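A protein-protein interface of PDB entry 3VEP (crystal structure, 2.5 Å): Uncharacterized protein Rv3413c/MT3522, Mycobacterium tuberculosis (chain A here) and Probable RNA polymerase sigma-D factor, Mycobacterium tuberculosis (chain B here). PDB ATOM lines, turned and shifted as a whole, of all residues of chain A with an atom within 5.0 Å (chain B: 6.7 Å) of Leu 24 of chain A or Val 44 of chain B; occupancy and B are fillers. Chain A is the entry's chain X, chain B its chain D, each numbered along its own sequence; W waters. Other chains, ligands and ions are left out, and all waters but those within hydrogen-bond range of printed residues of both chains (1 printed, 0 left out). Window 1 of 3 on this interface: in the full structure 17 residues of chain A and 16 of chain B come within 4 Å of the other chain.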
ATOM      1  N   THR A  20      37.524 -29.109  28.057  1.00  0.00           N
ATOM      2  CA  THR A  20      36.223 -28.565  27.698  1.00  0.00           C
ATOM      3  C   THR A  20      35.873 -29.030  26.258  1.00  0.00           C
ATOM      4  O   THR A  20      34.743 -29.464  25.973  1.00  0.00           O
ATOM      5  CB  THR A  20      36.198 -27.000  27.840  1.00  0.00           C
ATOM      6  OG1 THR A  20      37.099 -26.603  28.865  1.00  0.00           O
ATOM      7  CG2 THR A  20      34.858 -26.515  28.253  1.00  0.00           C
ATOM      8  N   ASP A  21      36.850 -28.943  25.357  1.00  0.00           N
ATOM      9  CA  ASP A  21      36.627 -29.322  23.968  1.00  0.00           C
ATOM     10  C   ASP A  21      36.137 -30.754  23.901  1.00  0.00           C
ATOM     11  O   ASP A  21      35.181 -31.069  23.186  1.00  0.00           O
ATOM     12  CB  ASP A  21      37.916 -29.204  23.172  1.00  0.00           C
ATOM     13  CG  ASP A  21      37.679 -29.069  21.700  1.00  0.00           C
ATOM     14  OD1 ASP A  21      36.665 -28.479  21.287  1.00  0.00           O
ATOM     15  OD2 ASP A  21      38.527 -29.549  20.939  1.00  0.00           O
ATOM     16  N   LEU A  22      36.785 -31.631  24.656  1.00  0.00           N
ATOM     17  CA  LEU A  22      36.349 -33.008  24.728  1.00  0.00           C
ATOM     18  C   LEU A  22      34.946 -33.147  25.325  1.00  0.00           C
ATOM     19  O   LEU A  22      34.121 -33.891  24.788  1.00  0.00           O
ATOM     20  CB  LEU A  22      37.362 -33.825  25.502  1.00  0.00           C
ATOM     21  CG  LEU A  22      38.285 -34.542  24.511  1.00  0.00           C
ATOM     22  CD1 LEU A  22      38.915 -33.593  23.478  1.00  0.00           C
ATOM     23  CD2 LEU A  22      39.319 -35.406  25.195  1.00  0.00           C
ATOM     24  N   LEU A  23      34.647 -32.421  26.405  1.00  0.00           N
ATOM     25  CA  LEU A  23      33.306 -32.498  26.983  1.00  0.00           C
ATOM     26  C   LEU A  23      32.228 -32.091  25.963  1.00  0.00           C
ATOM     27  O   LEU A  23      31.258 -32.823  25.750  1.00  0.00           O
ATOM     28  CB  LEU A  23      33.184 -31.634  28.231  1.00  0.00           C
ATOM     29  CG  LEU A  23      31.896 -31.806  29.049  1.00  0.00           C
ATOM     30  CD1 LEU A  23      31.159 -30.512  29.327  1.00  0.00           C
ATOM     31  CD2 LEU A  23      30.940 -32.939  28.579  1.00  0.00           C
ATOM     32  N   LEU A  24      32.400 -30.920  25.348  1.00  0.00           N
ATOM     33  CA  LEU A  24      31.494 -30.484  24.284  1.00  0.00           C
ATOM     34  C   LEU A  24      31.401 -31.505  23.112  1.00  0.00           C
ATOM     35  O   LEU A  24      30.316 -31.698  22.554  1.00  0.00           O
ATOM     36  CB  LEU A  24      31.854 -29.086  23.783  1.00  0.00           C
ATOM     37  CG  LEU A  24      31.725 -27.976  24.848  1.00  0.00           C
ATOM     38  CD1 LEU A  24      32.091 -26.628  24.292  1.00  0.00           C
ATOM     39  CD2 LEU A  24      30.319 -27.879  25.450  1.00  0.00           C
ATOM     40  N   ASP A  25      32.511 -32.162  22.761  1.00  0.00           N
ATOM     41  CA  ASP A  25      32.472 -33.142  21.678  1.00  0.00           C
ATOM     42  C   ASP A  25      31.598 -34.327  22.089  1.00  0.00           C
ATOM     43  O   ASP A  25      30.890 -34.891  21.253  1.00  0.00           O
ATOM     44  CB  ASP A  25      33.869 -33.676  21.308  1.00  0.00           C
ATOM     45  CG  ASP A  25      34.696 -32.701  20.442  1.00  0.00           C
ATOM     46  OD1 ASP A  25      34.140 -31.712  19.920  1.00  0.00           O
ATOM     47  OD2 ASP A  25      35.928 -32.936  20.291  1.00  0.00           O
ATOM     48  N   ALA A  26      31.655 -34.711  23.367  1.00  0.00           N
ATOM     49  CA  ALA A  26      30.838 -35.807  23.879  1.00  0.00           C
ATOM     50  C   ALA A  26      29.374 -35.397  23.952  1.00  0.00           C
ATOM     51  O   ALA A  26      28.483 -36.156  23.570  1.00  0.00           O
ATOM     52  CB  ALA A  26      31.326 -36.252  25.225  1.00  0.00           C
ATOM     53  N   LEU A  27      29.129 -34.189  24.444  1.00  0.00           N
ATOM     54  CA  LEU A  27      27.775 -33.656  24.451  1.00  0.00           C
ATOM     55  C   LEU A  27      27.192 -33.714  23.053  1.00  0.00           C
ATOM     56  O   LEU A  27      26.050 -34.077  22.876  1.00  0.00           O
ATOM     57  CB  LEU A  27      27.761 -32.224  24.967  1.00  0.00           C
ATOM     58  CG  LEU A  27      27.857 -32.230  26.507  1.00  0.00           C
ATOM     59  CD1 LEU A  27      28.122 -30.849  27.134  1.00  0.00           C
ATOM     60  CD2 LEU A  27      26.684 -32.933  27.183  1.00  0.00           C
ATOM     61  N   ALA A  28      27.990 -33.347  22.066  1.00  0.00           N
ATOM     62  CA  ALA A  28      27.505 -33.179  20.706  1.00  0.00           C
ATOM     63  C   ALA A  28      27.130 -34.521  20.079  1.00  0.00           C
ATOM     64  O   ALA A  28      26.212 -34.597  19.271  1.00  0.00           O
ATOM     65  CB  ALA A  28      28.541 -32.489  19.854  1.00  0.00           C
ATOM     66  N   LEU A  47      22.431 -29.716  29.760  1.00  0.00           N
ATOM     67  CA  LEU A  47      22.803 -29.388  28.397  1.00  0.00           C
ATOM     68  C   LEU A  47      22.316 -30.436  27.424  1.00  0.00           C
ATOM     69  O   LEU A  47      21.892 -30.120  26.317  1.00  0.00           O
ATOM     70  CB  LEU A  47      24.317 -29.258  28.280  1.00  0.00           C
ATOM     71  CG  LEU A  47      24.891 -27.936  28.788  1.00  0.00           C
ATOM     72  CD1 LEU A  47      26.433 -28.006  29.035  1.00  0.00           C
ATOM     73  CD2 LEU A  47      24.529 -26.822  27.825  1.00  0.00           C
ATOM     74  N   TRP A  50      18.683 -30.054  26.769  1.00  0.00           N
ATOM     75  CA  TRP A  50      18.501 -28.817  26.033  1.00  0.00           C
ATOM     76  C   TRP A  50      18.888 -29.004  24.575  1.00  0.00           C
ATOM     77  O   TRP A  50      18.192 -28.555  23.678  1.00  0.00           O
ATOM     78  CB  TRP A  50      19.342 -27.748  26.721  1.00  0.00           C
ATOM     79  CG  TRP A  50      19.580 -26.498  25.967  1.00  0.00           C
ATOM     80  CD1 TRP A  50      18.709 -25.453  25.799  1.00  0.00           C
ATOM     81  CD2 TRP A  50      20.805 -26.109  25.334  1.00  0.00           C
ATOM     82  NE1 TRP A  50      19.320 -24.445  25.084  1.00  0.00           N
ATOM     83  CE2 TRP A  50      20.601 -24.825  24.777  1.00  0.00           C
ATOM     84  CE3 TRP A  50      22.049 -26.729  25.166  1.00  0.00           C
ATOM     85  CZ2 TRP A  50      21.595 -24.151  24.066  1.00  0.00           C
ATOM     86  CZ3 TRP A  50      23.039 -26.055  24.463  1.00  0.00           C
ATOM     87  CH2 TRP A  50      22.808 -24.779  23.924  1.00  0.00           C
ATOM     88  N   ARG A  51      20.011 -29.681  24.372  1.00  0.00           N
ATOM     89  CA  ARG A  51      20.470 -30.161  23.081  1.00  0.00           C
ATOM     90  C   ARG A  51      19.339 -30.927  22.403  1.00  0.00           C
ATOM     91  O   ARG A  51      18.981 -30.644  21.260  1.00  0.00           O
ATOM     92  CB  ARG A  51      21.678 -31.104  23.293  1.00  0.00           C
ATOM     93  CG  ARG A  51      22.265 -31.781  22.034  1.00  0.00           C
ATOM     94  CD  ARG A  51      23.005 -33.093  22.362  1.00  0.00           C
ATOM     95  NE  ARG A  51      22.204 -33.996  23.184  1.00  0.00           N
ATOM     96  CZ  ARG A  51      22.657 -34.716  24.204  1.00  0.00           C
ATOM     97  NH1 ARG A  51      23.930 -34.674  24.579  1.00  0.00           N
ATOM     98  NH2 ARG A  51      21.812 -35.477  24.880  1.00  0.00           N
ATOM     99  N   ARG A  55      17.027 -29.740  19.117  1.00  0.00           N
ATOM    100  CA  ARG A  55      17.246 -30.473  17.883  1.00  0.00           C
ATOM    101  C   ARG A  55      15.882 -30.950  17.421  1.00  0.00           C
ATOM    102  O   ARG A  55      15.610 -31.131  16.230  1.00  0.00           O
ATOM    103  CB  ARG A  55      18.177 -31.670  18.127  1.00  0.00           C
ATOM    104  CG  ARG A  55      19.655 -31.403  17.840  1.00  0.00           C
ATOM    105  CD  ARG A  55      20.490 -32.555  18.370  1.00  0.00           C
ATOM    106  NE  ARG A  55      21.913 -32.237  18.499  1.00  0.00           N
ATOM    107  CZ  ARG A  55      22.879 -33.152  18.638  1.00  0.00           C
ATOM    108  NH1 ARG A  55      22.590 -34.447  18.660  1.00  0.00           N
ATOM    109  NH2 ARG A  55      24.138 -32.778  18.748  1.00  0.00           N
ATOM    110  N   ILE B  39      28.373 -20.066  19.916  1.00  0.00           N
ATOM    111  CA  ILE B  39      29.360 -21.133  19.820  1.00  0.00           C
ATOM    112  C   ILE B  39      28.932 -22.417  20.529  1.00  0.00           C
ATOM    113  O   ILE B  39      29.200 -23.512  20.043  1.00  0.00           O
ATOM    114  CB  ILE B  39      30.709 -20.656  20.391  1.00  0.00           C
ATOM    115  CG1 ILE B  39      31.280 -19.523  19.535  1.00  0.00           C
ATOM    116  CG2 ILE B  39      31.692 -21.813  20.477  1.00  0.00           C
ATOM    117  CD1 ILE B  39      32.461 -18.820  20.165  1.00  0.00           C
ATOM    118  N   LEU B  40      28.276 -22.275  21.675  1.00  0.00           N
ATOM    119  CA  LEU B  40      27.808 -23.430  22.464  1.00  0.00           C
ATOM    120  C   LEU B  40      26.721 -24.152  21.713  1.00  0.00           C
ATOM    121  O   LEU B  40      26.651 -25.392  21.704  1.00  0.00           O
ATOM    122  CB  LEU B  40      27.285 -23.015  23.862  1.00  0.00           C
ATOM    123  CG  LEU B  40      28.350 -22.576  24.881  1.00  0.00           C
ATOM    124  CD1 LEU B  40      27.766 -22.343  26.269  1.00  0.00           C
ATOM    125  CD2 LEU B  40      29.464 -23.609  24.960  1.00  0.00           C
ATOM    126  N   ILE B  41      25.863 -23.353  21.093  1.00  0.00           N
ATOM    127  CA  ILE B  41      24.771 -23.852  20.284  1.00  0.00           C
ATOM    128  C   ILE B  41      25.337 -24.656  19.107  1.00  0.00           C
ATOM    129  O   ILE B  41      24.992 -25.812  18.897  1.00  0.00           O
ATOM    130  CB  ILE B  41      23.888 -22.697  19.776  1.00  0.00           C
ATOM    131  CG1 ILE B  41      23.161 -22.027  20.945  1.00  0.00           C
ATOM    132  CG2 ILE B  41      22.893 -23.202  18.743  1.00  0.00           C
ATOM    133  CD1 ILE B  41      22.482 -20.727  20.576  1.00  0.00           C
ATOM    134  N   LEU B  42      26.234 -24.054  18.346  1.00  0.00           N
ATOM    135  CA  LEU B  42      26.790 -24.779  17.237  1.00  0.00           C
ATOM    136  C   LEU B  42      27.475 -26.050  17.722  1.00  0.00           C
ATOM    137  O   LEU B  42      27.277 -27.118  17.162  1.00  0.00           O
ATOM    138  CB  LEU B  42      27.722 -23.887  16.404  1.00  0.00           C
ATOM    139  CG  LEU B  42      27.083 -22.632  15.746  1.00  0.00           C
ATOM    140  CD1 LEU B  42      28.070 -21.793  14.987  1.00  0.00           C
ATOM    141  CD2 LEU B  42      25.983 -23.011  14.802  1.00  0.00           C
ATOM    142  N   ARG B  43      28.261 -25.956  18.782  1.00  0.00           N
ATOM    143  CA  ARG B  43      29.043 -27.105  19.200  1.00  0.00           C
ATOM    144  C   ARG B  43      28.202 -28.245  19.728  1.00  0.00           C
ATOM    145  O   ARG B  43      28.541 -29.391  19.545  1.00  0.00           O
ATOM    146  CB  ARG B  43      30.075 -26.699  20.246  1.00  0.00           C
ATOM    147  CG  ARG B  43      31.130 -25.753  19.696  1.00  0.00           C
ATOM    148  CD  ARG B  43      32.195 -26.526  18.994  1.00  0.00           C
ATOM    149  NE  ARG B  43      33.029 -27.223  19.958  1.00  0.00           N
ATOM    150  CZ  ARG B  43      33.008 -28.538  20.153  1.00  0.00           C
ATOM    151  NH1 ARG B  43      32.187 -29.295  19.422  1.00  0.00           N
ATOM    152  NH2 ARG B  43      33.818 -29.082  21.077  1.00  0.00           N
ATOM    153  N   VAL B  44      27.104 -27.917  20.379  1.00  0.00           N
ATOM    154  CA  VAL B  44      26.347 -28.895  21.133  1.00  0.00           C
ATOM    155  C   VAL B  44      25.070 -29.320  20.417  1.00  0.00           C
ATOM    156  O   VAL B  44      24.774 -30.504  20.304  1.00  0.00           O
ATOM    157  CB  VAL B  44      26.029 -28.343  22.528  1.00  0.00           C
ATOM    158  CG1 VAL B  44      25.044 -29.242  23.261  1.00  0.00           C
ATOM    159  CG2 VAL B  44      27.336 -28.179  23.302  1.00  0.00           C
ATOM    160  N   VAL B  45      24.329 -28.339  19.928  1.00  0.00           N
ATOM    161  CA  VAL B  45      23.034 -28.563  19.312  1.00  0.00           C
ATOM    162  C   VAL B  45      23.191 -28.957  17.846  1.00  0.00           C
ATOM    163  O   VAL B  45      22.583 -29.911  17.381  1.00  0.00           O
ATOM    164  CB  VAL B  45      22.169 -27.310  19.401  1.00  0.00           C
ATOM    165  CG1 VAL B  45      20.847 -27.544  18.674  1.00  0.00           C
ATOM    166  CG2 VAL B  45      21.947 -26.919  20.881  1.00  0.00           C
ATOM    167  N   VAL B  46      24.030 -28.250  17.117  1.00  0.00           N
ATOM    168  CA  VAL B  46      24.293 -28.695  15.762  1.00  0.00           C
ATOM    169  C   VAL B  46      25.273 -29.865  15.808  1.00  0.00           C
ATOM    170  O   VAL B  46      25.099 -30.869  15.091  1.00  0.00           O
ATOM    171  CB  VAL B  46      24.800 -27.577  14.839  1.00  0.00           C
ATOM    172  CG1 VAL B  46      25.061 -28.136  13.470  1.00  0.00           C
ATOM    173  CG2 VAL B  46      23.781 -26.457  14.751  1.00  0.00           C
ATOM    174  N   GLY B  47      26.260 -29.743  16.705  1.00  0.00           N
ATOM    175  CA  GLY B  47      27.276 -30.760  16.889  1.00  0.00           C
ATOM    176  C   GLY B  47      28.488 -30.490  16.036  1.00  0.00           C
ATOM    177  O   GLY B  47      29.263 -31.396  15.707  1.00  0.00           O
ATOM    178  N   LEU B  48      28.657 -29.229  15.660  1.00  0.00           N
ATOM    179  CA  LEU B  48      29.849 -28.829  14.936  1.00  0.00           C
ATOM    180  C   LEU B  48      31.116 -29.024  15.788  1.00  0.00           C
ATOM    181  O   LEU B  48      31.071 -28.946  17.008  1.00  0.00           O
ATOM    182  CB  LEU B  48      29.720 -27.388  14.484  1.00  0.00           C
ATOM    183  CG  LEU B  48      29.386 -27.067  13.025  1.00  0.00           C
ATOM    184  CD1 LEU B  48      28.450 -28.108  12.355  1.00  0.00           C
ATOM    185  CD2 LEU B  48      28.804 -25.695  12.953  1.00  0.00           C
ATOM    186  N   THR B  53      33.065 -24.961  13.748  1.00  0.00           N
ATOM    187  CA  THR B  53      32.437 -23.842  14.425  1.00  0.00           C
ATOM    188  C   THR B  53      33.220 -22.562  14.083  1.00  0.00           C
ATOM    189  O   THR B  53      32.620 -21.526  13.763  1.00  0.00           O
ATOM    190  CB  THR B  53      32.391 -24.058  15.961  1.00  0.00           C
ATOM    191  OG1 THR B  53      31.525 -25.158  16.270  1.00  0.00           O
ATOM    192  CG2 THR B  53      31.877 -22.808  16.655  1.00  0.00           C
ATOM    193  N   GLN B  68      34.486 -21.063  24.032  1.00  0.00           N
ATOM    194  CA  GLN B  68      33.582 -22.114  24.460  1.00  0.00           C
ATOM    195  C   GLN B  68      33.905 -22.499  25.911  1.00  0.00           C
ATOM    196  O   GLN B  68      33.007 -22.839  26.662  1.00  0.00           O
ATOM    197  CB  GLN B  68      33.585 -23.313  23.489  1.00  0.00           C
ATOM    198  CG  GLN B  68      34.619 -24.433  23.787  1.00  0.00           C
ATOM    199  CD  GLN B  68      34.994 -25.293  22.547  1.00  0.00           C
ATOM    200  OE1 GLN B  68      34.342 -25.237  21.489  1.00  0.00           O
ATOM    201  NE2 GLN B  68      36.053 -26.099  22.695  1.00  0.00           N
ATOM    202  N   HIS B  69      35.188 -22.419  26.286  1.00  0.00           N
ATOM    203  CA  HIS B  69      35.626 -22.700  27.638  1.00  0.00           C
ATOM    204  C   HIS B  69      35.101 -21.629  28.578  1.00  0.00           C
ATOM    205  O   HIS B  69      34.470 -21.924  29.589  1.00  0.00           O
ATOM    206  CB  HIS B  69      37.139 -22.766  27.731  1.00  0.00           C
ATOM    207  CG  HIS B  69      37.639 -22.974  29.115  1.00  0.00           C
ATOM    208  ND1 HIS B  69      37.520 -24.191  29.778  1.00  0.00           N
ATOM    209  CD2 HIS B  69      38.224 -22.135  30.010  1.00  0.00           C
ATOM    210  CE1 HIS B  69      38.033 -24.086  30.983  1.00  0.00           C
ATOM    211  NE2 HIS B  69      38.467 -22.840  31.150  1.00  0.00           N
ATOM    212  N   LEU B  72      31.546 -22.069  29.170  1.00  0.00           N
ATOM    213  CA  LEU B  72      31.223 -23.190  30.020  1.00  0.00           C
ATOM    214  C   LEU B  72      31.377 -22.799  31.475  1.00  0.00           C
ATOM    215  O   LEU B  72      30.513 -23.122  32.288  1.00  0.00           O
ATOM    216  CB  LEU B  72      32.103 -24.392  29.687  1.00  0.00           C
ATOM    217  CG  LEU B  72      31.462 -25.780  29.672  1.00  0.00           C
ATOM    218  CD1 LEU B  72      32.145 -26.692  30.679  1.00  0.00           C
ATOM    219  CD2 LEU B  72      29.971 -25.741  29.903  1.00  0.00           C
HETATM  220  O   HOH W   1      36.240 -29.804  18.731  1.00  0.00           O
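The guanidinium group of Arg 55 of chain A lies within hydrogen-bond range of the backbone carbonyl oxygen of Val 44 of chain B (2.8 Å).
The side-chain carboxylate of Asp 21 of chain A is in salt-bridge range of the guanidinium group of Arg 43 of chain B (2.9 Å).
The guanidinium group of Arg 55 of chain A lies within hydrogen-bond range of the backbone carbonyl oxygen of Val 45 of chain B (2.7 Å).
NE2 of Gln 68 of chain B is in hydrogen-bond range of OD1 of Asp 21 of chain A (2.8 Å).
The side-chain carboxylate (OD1) of Asp 25 of chain A is in salt-bridge range of the guanidinium group (NH2) of Arg 43 of chain B.
OG1 of Thr 20 of chain A is in hydrogen-bond range of ND1 of His 69 of chain B, 2.6 Å away.
NH2 of Arg 55 of chain A lies within hydrogen-bond range of O of Ala 28 of chain A, 2.8 Å away.
The backbone carbonyl oxygen of Leu 27 of chain A sits at hydrogen-bond distance from the guanidinium group of Arg 51 of chain A, at 2.8 Å.
The backbone carbonyl oxygen of Leu 42 of chain B is in hydrogen-bond range of the backbone NH of Gly 47 of chain B (2.9 Å).
NH1 of Arg 43 of chain B lies within hydrogen-bond range of O of Leu 48 of chain B (2.7 Å).
The guanidinium group (NE) of Arg 43 of chain B is in hydrogen-bond range of the side-chain amide oxygen (OE1) of Gln 68 of chain B (2.8 Å).
Leu 22 of chain A touches none of the printed residues of chain B.
Leu 24 of chain A touches three residues of chain B.
Ala 26 of chain A touches none of the printed residues of chain B.
Of the printed residues of chain B, Arg 55 of chain A touches Val 44 (2.8 Å) and Val 45 (2.7 Å).
Of chain A, only Leu 24 (3.7 Å), Ala 28 (3.8 Å), Trp 50 (3.95 Å), Arg 51 (3.3 Å) and Arg 55 (2.8 Å) come within 4 Å of Val 44 of chain B.
Printed residues of chain A within 4 Å of Val 45 of chain B: Trp 50 and Arg 55.
Printed residues of chain A within 4 Å of Gln 68 of chain B: Asp 21 (2.8 Å) and Leu 24 (3.4 Å).
The nearest residue of chain B that does not touch Leu 24 of chain A is Leu 40 of chain B (4.1 Å).
Of the 14 printed residues of chain B, 7 touch a printed residue of chain A.
Hydrophobic or aromatic side chains of chain B within 4 Å of the printed part of chain A: Val 44, Val 45, His 69 and Leu 72.
Among the printed residues, 16 pairs touch across the chains.
Water W1 lies within hydrogen-bond range of OD1 of Asp 21 of chain A (2.9 Å), OD1 of Asp 25 of chain A (3.1 Å) and NH2 of Arg 43 of chain B (3.4 Å).
CG2 of Thr 20 of chain A touches CD1 of Leu 72 of chain B (3.6 Å).
NH2 of Arg 43 of chain B touches CB of Leu 24 of chain A, at 3.3 Å.
Val 44 of chain B touches Leu 24 of chain A.
CG of Gln 68 of chain B touches CD1 of Leu 24 of chain A, 3.4 Å away.
Arg 43 of chain B touches Ala 28 of chain A (O to CB, 3.1 Å).
Ala 28 of chain A touches Val 44 of chain B.
Ala 28 of chain A touches Gly 47 of chain B (CB to CA, 3.7 Å).
Trp 50 of chain A touches Val 44 of chain B.
Val 45 of chain B touches Trp 50 of chain A (CG2 to CH2, 3.8 Å).
Arg 51 of chain A touches Val 44 of chain B (CG to O, 3.3 Å).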
